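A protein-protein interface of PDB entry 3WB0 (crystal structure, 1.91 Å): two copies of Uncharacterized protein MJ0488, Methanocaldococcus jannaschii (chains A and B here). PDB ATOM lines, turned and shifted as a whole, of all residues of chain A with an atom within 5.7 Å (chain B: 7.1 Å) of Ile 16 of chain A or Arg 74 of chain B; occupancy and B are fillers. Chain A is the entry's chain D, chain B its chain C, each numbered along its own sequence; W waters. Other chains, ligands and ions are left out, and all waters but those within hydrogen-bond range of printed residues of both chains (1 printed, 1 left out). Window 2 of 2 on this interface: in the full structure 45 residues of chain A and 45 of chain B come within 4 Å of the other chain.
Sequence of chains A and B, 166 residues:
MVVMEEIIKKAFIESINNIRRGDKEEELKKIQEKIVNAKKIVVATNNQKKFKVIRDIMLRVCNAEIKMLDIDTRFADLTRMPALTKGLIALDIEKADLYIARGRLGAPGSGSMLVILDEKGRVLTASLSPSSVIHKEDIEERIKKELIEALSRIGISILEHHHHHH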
ATOM      1  N   ALA A  11     -11.590   8.165  13.996  1.00  0.00           N
ATOM      2  CA  ALA A  11     -10.755   8.406  15.206  1.00  0.00           C
ATOM      3  C   ALA A  11      -9.844   9.615  14.973  1.00  0.00           C
ATOM      4  O   ALA A  11      -9.652  10.481  15.870  1.00  0.00           O
ATOM      5  CB  ALA A  11      -9.911   7.185  15.513  1.00  0.00           C
ATOM      6  N   PHE A  12      -9.246   9.671  13.770  1.00  0.00           N
ATOM      7  CA  PHE A  12      -8.281  10.769  13.475  1.00  0.00           C
ATOM      8  C   PHE A  12      -8.976  12.152  13.451  1.00  0.00           C
ATOM      9  O   PHE A  12      -8.440  13.174  13.926  1.00  0.00           O
ATOM     10  CB  PHE A  12      -7.585  10.503  12.158  1.00  0.00           C
ATOM     11  CG  PHE A  12      -6.462   9.476  12.253  1.00  0.00           C
ATOM     12  CD1 PHE A  12      -6.258   8.696  13.407  1.00  0.00           C
ATOM     13  CD2 PHE A  12      -5.550   9.311  11.142  1.00  0.00           C
ATOM     14  CE1 PHE A  12      -5.238   7.752  13.431  1.00  0.00           C
ATOM     15  CE2 PHE A  12      -4.526   8.384  11.202  1.00  0.00           C
ATOM     16  CZ  PHE A  12      -4.371   7.621  12.346  1.00  0.00           C
ATOM     17  N   ILE A  13     -10.170  12.190  12.871  1.00  0.00           N
ATOM     18  CA  ILE A  13     -10.956  13.414  12.883  1.00  0.00           C
ATOM     19  C   ILE A  13     -11.331  13.820  14.312  1.00  0.00           C
ATOM     20  O   ILE A  13     -11.228  15.001  14.712  1.00  0.00           O
ATOM     21  CB  ILE A  13     -12.203  13.248  12.004  1.00  0.00           C
ATOM     22  CG1 ILE A  13     -11.818  13.258  10.498  1.00  0.00           C
ATOM     23  CG2 ILE A  13     -13.216  14.344  12.347  1.00  0.00           C
ATOM     24  CD1 ILE A  13     -12.989  12.794   9.578  1.00  0.00           C
ATOM     25  N   GLU A  14     -11.702  12.852  15.123  1.00  0.00           N
ATOM     26  CA  GLU A  14     -12.031  13.205  16.513  1.00  0.00           C
ATOM     27  C   GLU A  14     -10.830  13.773  17.265  1.00  0.00           C
ATOM     28  O   GLU A  14     -10.952  14.652  18.130  1.00  0.00           O
ATOM     29  CB  GLU A  14     -12.585  11.995  17.280  1.00  0.00           C
ATOM     30  CG  GLU A  14     -13.932  11.432  16.888  1.00  0.00           C
ATOM     31  CD  GLU A  14     -14.299  10.272  17.811  1.00  0.00           C
ATOM     32  OE1 GLU A  14     -13.369   9.533  18.266  1.00  0.00           O
ATOM     33  OE2 GLU A  14     -15.519  10.097  18.127  1.00  0.00           O
ATOM     34  N   SER A  15      -9.635  13.301  16.913  1.00  0.00           N
ATOM     35  CA  SER A  15      -8.452  13.700  17.633  1.00  0.00           C
ATOM     36  C   SER A  15      -8.111  15.115  17.166  1.00  0.00           C
ATOM     37  O   SER A  15      -7.867  16.013  17.956  1.00  0.00           O
ATOM     38  CB  SER A  15      -7.345  12.694  17.316  1.00  0.00           C
ATOM     39  OG  SER A  15      -7.464  11.591  18.213  1.00  0.00           O
ATOM     40  N   ILE A  16      -8.154  15.321  15.860  1.00  0.00           N
ATOM     41  CA  ILE A  16      -7.840  16.625  15.335  1.00  0.00           C
ATOM     42  C   ILE A  16      -8.749  17.684  15.966  1.00  0.00           C
ATOM     43  O   ILE A  16      -8.293  18.774  16.352  1.00  0.00           O
ATOM     44  CB  ILE A  16      -7.954  16.597  13.804  1.00  0.00           C
ATOM     45  CG1 ILE A  16      -6.858  15.713  13.178  1.00  0.00           C
ATOM     46  CG2 ILE A  16      -8.031  17.995  13.196  1.00  0.00           C
ATOM     47  CD1 ILE A  16      -7.208  15.474  11.710  1.00  0.00           C
ATOM     48  N   ASN A  17     -10.011  17.335  16.150  1.00  0.00           N
ATOM     49  CA  ASN A  17     -11.000  18.357  16.572  1.00  0.00           C
ATOM     50  C   ASN A  17     -11.331  18.346  18.040  1.00  0.00           C
ATOM     51  O   ASN A  17     -12.337  18.929  18.462  1.00  0.00           O
ATOM     52  CB  ASN A  17     -12.234  18.243  15.666  1.00  0.00           C
ATOM     53  CG  ASN A  17     -11.887  18.545  14.230  1.00  0.00           C
ATOM     54  OD1 ASN A  17     -11.702  19.703  13.901  1.00  0.00           O
ATOM     55  ND2 ASN A  17     -11.836  17.521  13.351  1.00  0.00           N
ATOM     56  N   ASN A  18     -10.453  17.707  18.819  1.00  0.00           N
ATOM     57  CA  ASN A  18     -10.523  17.726  20.283  1.00  0.00           C
ATOM     58  C   ASN A  18     -11.833  17.167  20.841  1.00  0.00           C
ATOM     59  O   ASN A  18     -12.353  17.635  21.880  1.00  0.00           O
ATOM     60  CB  ASN A  18     -10.164  19.115  20.879  1.00  0.00           C
ATOM     61  CG  ASN A  18      -9.699  19.029  22.344  1.00  0.00           C
ATOM     62  OD1 ASN A  18      -9.126  18.036  22.759  1.00  0.00           O
ATOM     63  ND2 ASN A  18      -9.954  20.076  23.121  1.00  0.00           N
ATOM     64  N   ALA B  44       4.832  13.833  29.469  1.00  0.00           N
ATOM     65  CA  ALA B  44       4.558  14.247  28.072  1.00  0.00           C
ATOM     66  C   ALA B  44       3.074  14.470  27.797  1.00  0.00           C
ATOM     67  O   ALA B  44       2.417  13.824  26.917  1.00  0.00           O
ATOM     68  CB  ALA B  44       5.182  13.264  27.056  1.00  0.00           C
ATOM     69  N   ASN B  46      -0.196  17.766  28.693  1.00  0.00           N
ATOM     70  CA  ASN B  46      -0.589  19.036  29.286  1.00  0.00           C
ATOM     71  C   ASN B  46      -1.802  18.809  30.202  1.00  0.00           C
ATOM     72  O   ASN B  46      -2.386  19.748  30.739  1.00  0.00           O
ATOM     73  CB  ASN B  46      -0.802  20.118  28.214  1.00  0.00           C
ATOM     74  CG  ASN B  46      -2.159  20.017  27.524  1.00  0.00           C
ATOM     75  OD1 ASN B  46      -2.777  18.952  27.475  1.00  0.00           O
ATOM     76  ND2 ASN B  46      -2.620  21.145  26.964  1.00  0.00           N
ATOM     77  N   ILE B  71       2.153  22.235  25.632  1.00  0.00           N
ATOM     78  CA  ILE B  71       1.392  21.926  24.430  1.00  0.00           C
ATOM     79  C   ILE B  71       0.561  20.638  24.636  1.00  0.00           C
ATOM     80  O   ILE B  71       0.966  19.727  25.387  1.00  0.00           O
ATOM     81  CB  ILE B  71       2.268  21.821  23.167  1.00  0.00           C
ATOM     82  CG1 ILE B  71       3.203  20.610  23.239  1.00  0.00           C
ATOM     83  CG2 ILE B  71       3.031  23.122  22.923  1.00  0.00           C
ATOM     84  CD1 ILE B  71       3.919  20.311  21.921  1.00  0.00           C
ATOM     85  N   ASP B  72      -0.591  20.582  23.959  1.00  0.00           N
ATOM     86  CA  ASP B  72      -1.392  19.388  23.894  1.00  0.00           C
ATOM     87  C   ASP B  72      -0.718  18.397  22.950  1.00  0.00           C
ATOM     88  O   ASP B  72      -0.600  18.677  21.764  1.00  0.00           O
ATOM     89  CB  ASP B  72      -2.790  19.702  23.359  1.00  0.00           C
ATOM     90  CG  ASP B  72      -3.796  18.552  23.595  1.00  0.00           C
ATOM     91  OD1 ASP B  72      -3.389  17.432  23.976  1.00  0.00           O
ATOM     92  OD2 ASP B  72      -5.006  18.784  23.409  1.00  0.00           O
ATOM     93  N   THR B  73      -0.325  17.231  23.471  1.00  0.00           N
ATOM     94  CA  THR B  73       0.209  16.163  22.605  1.00  0.00           C
ATOM     95  C   THR B  73      -0.847  15.233  21.952  1.00  0.00           C
ATOM     96  O   THR B  73      -0.495  14.132  21.459  1.00  0.00           O
ATOM     97  CB  THR B  73       1.267  15.294  23.339  1.00  0.00           C
ATOM     98  OG1 THR B  73       0.643  14.632  24.431  1.00  0.00           O
ATOM     99  CG2 THR B  73       2.461  16.132  23.820  1.00  0.00           C
ATOM    100  N   ARG B  74      -2.118  15.642  21.937  1.00  0.00           N
ATOM    101  CA  ARG B  74      -3.174  14.778  21.339  1.00  0.00           C
ATOM    102  C   ARG B  74      -2.983  14.516  19.809  1.00  0.00           C
ATOM    103  O   ARG B  74      -3.423  13.494  19.264  1.00  0.00           O
ATOM    104  CB  ARG B  74      -4.576  15.322  21.639  1.00  0.00           C
ATOM    105  CG  ARG B  74      -4.982  16.471  20.723  1.00  0.00           C
ATOM    106  CD  ARG B  74      -6.448  16.773  20.855  1.00  0.00           C
ATOM    107  NE  ARG B  74      -6.878  17.850  19.920  1.00  0.00           N
ATOM    108  CZ  ARG B  74      -6.757  19.156  20.158  1.00  0.00           C
ATOM    109  NH1 ARG B  74      -6.189  19.575  21.286  1.00  0.00           N
ATOM    110  NH2 ARG B  74      -7.161  20.045  19.256  1.00  0.00           N
ATOM    111  N   PHE B  75      -2.312  15.424  19.137  1.00  0.00           N
ATOM    112  CA  PHE B  75      -1.980  15.213  17.713  1.00  0.00           C
ATOM    113  C   PHE B  75      -1.082  13.971  17.437  1.00  0.00           C
ATOM    114  O   PHE B  75      -1.096  13.418  16.325  1.00  0.00           O
ATOM    115  CB  PHE B  75      -1.455  16.523  17.116  1.00  0.00           C
ATOM    116  CG  PHE B  75      -2.334  17.725  17.459  1.00  0.00           C
ATOM    117  CD1 PHE B  75      -3.618  17.859  16.919  1.00  0.00           C
ATOM    118  CD2 PHE B  75      -1.906  18.691  18.392  1.00  0.00           C
ATOM    119  CE1 PHE B  75      -4.447  18.935  17.262  1.00  0.00           C
ATOM    120  CE2 PHE B  75      -2.735  19.764  18.743  1.00  0.00           C
ATOM    121  CZ  PHE B  75      -4.001  19.894  18.162  1.00  0.00           C
ATOM    122  N   ALA B  76      -0.320  13.522  18.438  1.00  0.00           N
ATOM    123  CA  ALA B  76       0.337  12.229  18.363  1.00  0.00           C
ATOM    124  C   ALA B  76      -0.667  11.107  18.003  1.00  0.00           C
ATOM    125  O   ALA B  76      -0.277  10.003  17.592  1.00  0.00           O
ATOM    126  CB  ALA B  76       0.956  11.948  19.728  1.00  0.00           C
ATOM    127  N   ASP B  77      -1.969  11.363  18.269  1.00  0.00           N
ATOM    128  CA  ASP B  77      -2.957  10.340  18.028  1.00  0.00           C
ATOM    129  C   ASP B  77      -3.214  10.042  16.568  1.00  0.00           C
ATOM    130  O   ASP B  77      -4.025   9.119  16.297  1.00  0.00           O
ATOM    131  CB  ASP B  77      -4.271  10.601  18.836  1.00  0.00           C
ATOM    132  CG  ASP B  77      -3.982  10.721  20.357  1.00  0.00           C
ATOM    133  OD1 ASP B  77      -2.962  10.156  20.797  1.00  0.00           O
ATOM    134  OD2 ASP B  77      -4.648  11.488  21.059  1.00  0.00           O
ATOM    135  N   LEU B  78      -2.563  10.771  15.625  1.00  0.00           N
ATOM    136  CA  LEU B  78      -2.666  10.373  14.188  1.00  0.00           C
ATOM    137  C   LEU B  78      -1.526   9.456  13.753  1.00  0.00           C
ATOM    138  O   LEU B  78      -1.495   9.011  12.579  1.00  0.00           O
ATOM    139  CB  LEU B  78      -2.710  11.589  13.272  1.00  0.00           C
ATOM    140  CG  LEU B  78      -3.978  12.470  13.256  1.00  0.00           C
ATOM    141  CD1 LEU B  78      -4.503  12.933  14.613  1.00  0.00           C
ATOM    142  CD2 LEU B  78      -3.670  13.723  12.399  1.00  0.00           C
ATOM    143  N   THR B  79      -0.596   9.146  14.669  1.00  0.00           N
ATOM    144  CA  THR B  79       0.585   8.367  14.283  1.00  0.00           C
ATOM    145  C   THR B  79       0.357   6.872  14.689  1.00  0.00           C
ATOM    146  O   THR B  79      -0.623   6.552  15.371  1.00  0.00           O
ATOM    147  CB  THR B  79       1.902   8.933  14.912  1.00  0.00           C
ATOM    148  OG1 THR B  79       1.932   8.635  16.321  1.00  0.00           O
ATOM    149  CG2 THR B  79       2.021  10.420  14.728  1.00  0.00           C
ATOM    150  N   PRO B  82       0.959   6.259  19.199  1.00  0.00           N
ATOM    151  CA  PRO B  82       0.768   7.532  19.814  1.00  0.00           C
ATOM    152  C   PRO B  82       1.561   7.786  21.106  1.00  0.00           C
ATOM    153  O   PRO B  82       2.047   8.924  21.258  1.00  0.00           O
ATOM    154  CB  PRO B  82      -0.778   7.617  20.016  1.00  0.00           C
ATOM    155  CG  PRO B  82      -1.258   6.884  18.781  1.00  0.00           C
ATOM    156  CD  PRO B  82      -0.327   5.682  18.770  1.00  0.00           C
ATOM    157  N   LYS B  86       4.285  10.761  21.560  1.00  0.00           N
ATOM    158  CA  LYS B  86       4.210  11.754  22.620  1.00  0.00           C
ATOM    159  C   LYS B  86       5.553  11.940  23.392  1.00  0.00           C
ATOM    160  O   LYS B  86       6.003  13.057  23.645  1.00  0.00           O
ATOM    161  CB  LYS B  86       3.108  11.343  23.622  1.00  0.00           C
ATOM    162  CG  LYS B  86       1.690  11.416  23.080  1.00  0.00           C
ATOM    163  CD  LYS B  86       0.738  11.049  24.239  1.00  0.00           C
ATOM    164  CE  LYS B  86      -0.734  10.953  23.919  1.00  0.00           C
ATOM    165  NZ  LYS B  86      -1.348  12.285  23.689  1.00  0.00           N
ATOM    166  N   ILE B  89       7.984  13.840  21.056  1.00  0.00           N
ATOM    167  CA  ILE B  89       7.664  15.279  21.023  1.00  0.00           C
ATOM    168  C   ILE B  89       8.280  15.977  22.274  1.00  0.00           C
ATOM    169  O   ILE B  89       8.935  16.997  22.131  1.00  0.00           O
ATOM    170  CB  ILE B  89       6.127  15.531  20.995  1.00  0.00           C
ATOM    171  CG1 ILE B  89       5.527  15.006  19.686  1.00  0.00           C
ATOM    172  CG2 ILE B  89       5.765  17.027  21.163  1.00  0.00           C
ATOM    173  CD1 ILE B  89       3.995  15.196  19.573  1.00  0.00           C
HETATM  174  O   HOH W   1      -7.010   9.255  17.338  1.00  0.00           O
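O of Ser 15 of chain A lies within hydrogen-bond range of NE of Arg 74 of chain B (2.9 Å). The guanidinium group of Arg 74 of chain B lies within hydrogen-bond range of the backbone carbonyl oxygen of Ile 16 of chain A (3.4 Å).
The side-chain carboxylate (OD2) of Asp 72 of chain B lies within salt-bridge range of the guanidinium group (NH1) of Arg 74 of chain B, 2.6 Å away. NZ of Lys 86 of chain B lies within salt-bridge range of OD1 of Asp 77 of chain B, at 3.9 Å. O of Ala 11 of chain A lies within hydrogen-bond range of OG of Ser 15 of chain A, at 3.4 Å.
Among the printed residues, merely in contact across the chains: Phe 12 of chain A with Leu 78 of chain B (3.2 Å), Phe 12 of chain A with Asp 77 of chain B (3.4 Å), Ser 15 of chain A with Asp 77 of chain B (3.4 Å), Asn 18 of chain A with Arg 74 of chain B (3.5 Å), Ile 16 of chain A with Leu 78 of chain B (3.8 Å), Ser 15 of chain A with Leu 78 of chain B (3.9 Å) and Ile 16 of chain A with Phe 75 of chain B (3.96 Å).
Ile 13 of chain A touches none of the printed residues of chain B. Printed residues of chain B within 4 Å of Ser 15 of chain A: Arg 74 (2.9 Å), Asp 77 (3.4 Å) and Leu 78 (3.9 Å). Of the printed residues of chain B, Ile 16 of chain A touches Arg 74, Phe 75 and Leu 78. Printed residues of chain A within 4 Å of Phe 75 of chain B: Ile 16. The nearest residue of chain B that does not touch Ile 16 of chain A is Asp 77 of chain B (6.8 Å).
Printed residues of chain B that touch a printed residue of chain A: Arg 74, Phe 75, Asp 77 and Leu 78. Hydrophobic or aromatic side chains of chain B within 4 Å of the printed part of chain A: Phe 75 and Leu 78. Among the printed residues, 9 pairs touch across the chains.
No position is printed for both chains. Of the 9 pairs that touch across the chains among the printed residues, none has its exchanged pair printed and touching as well.
Water W1 lies within hydrogen-bond range of the side-chain hydroxyl of Ser 15 of chain A (2.5 Å), the backbone carbonyl oxygen of Asp 77 of chain B (3.2 Å) and the backbone carbonyl oxygen of Ala 11 of chain A (3.3 Å).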
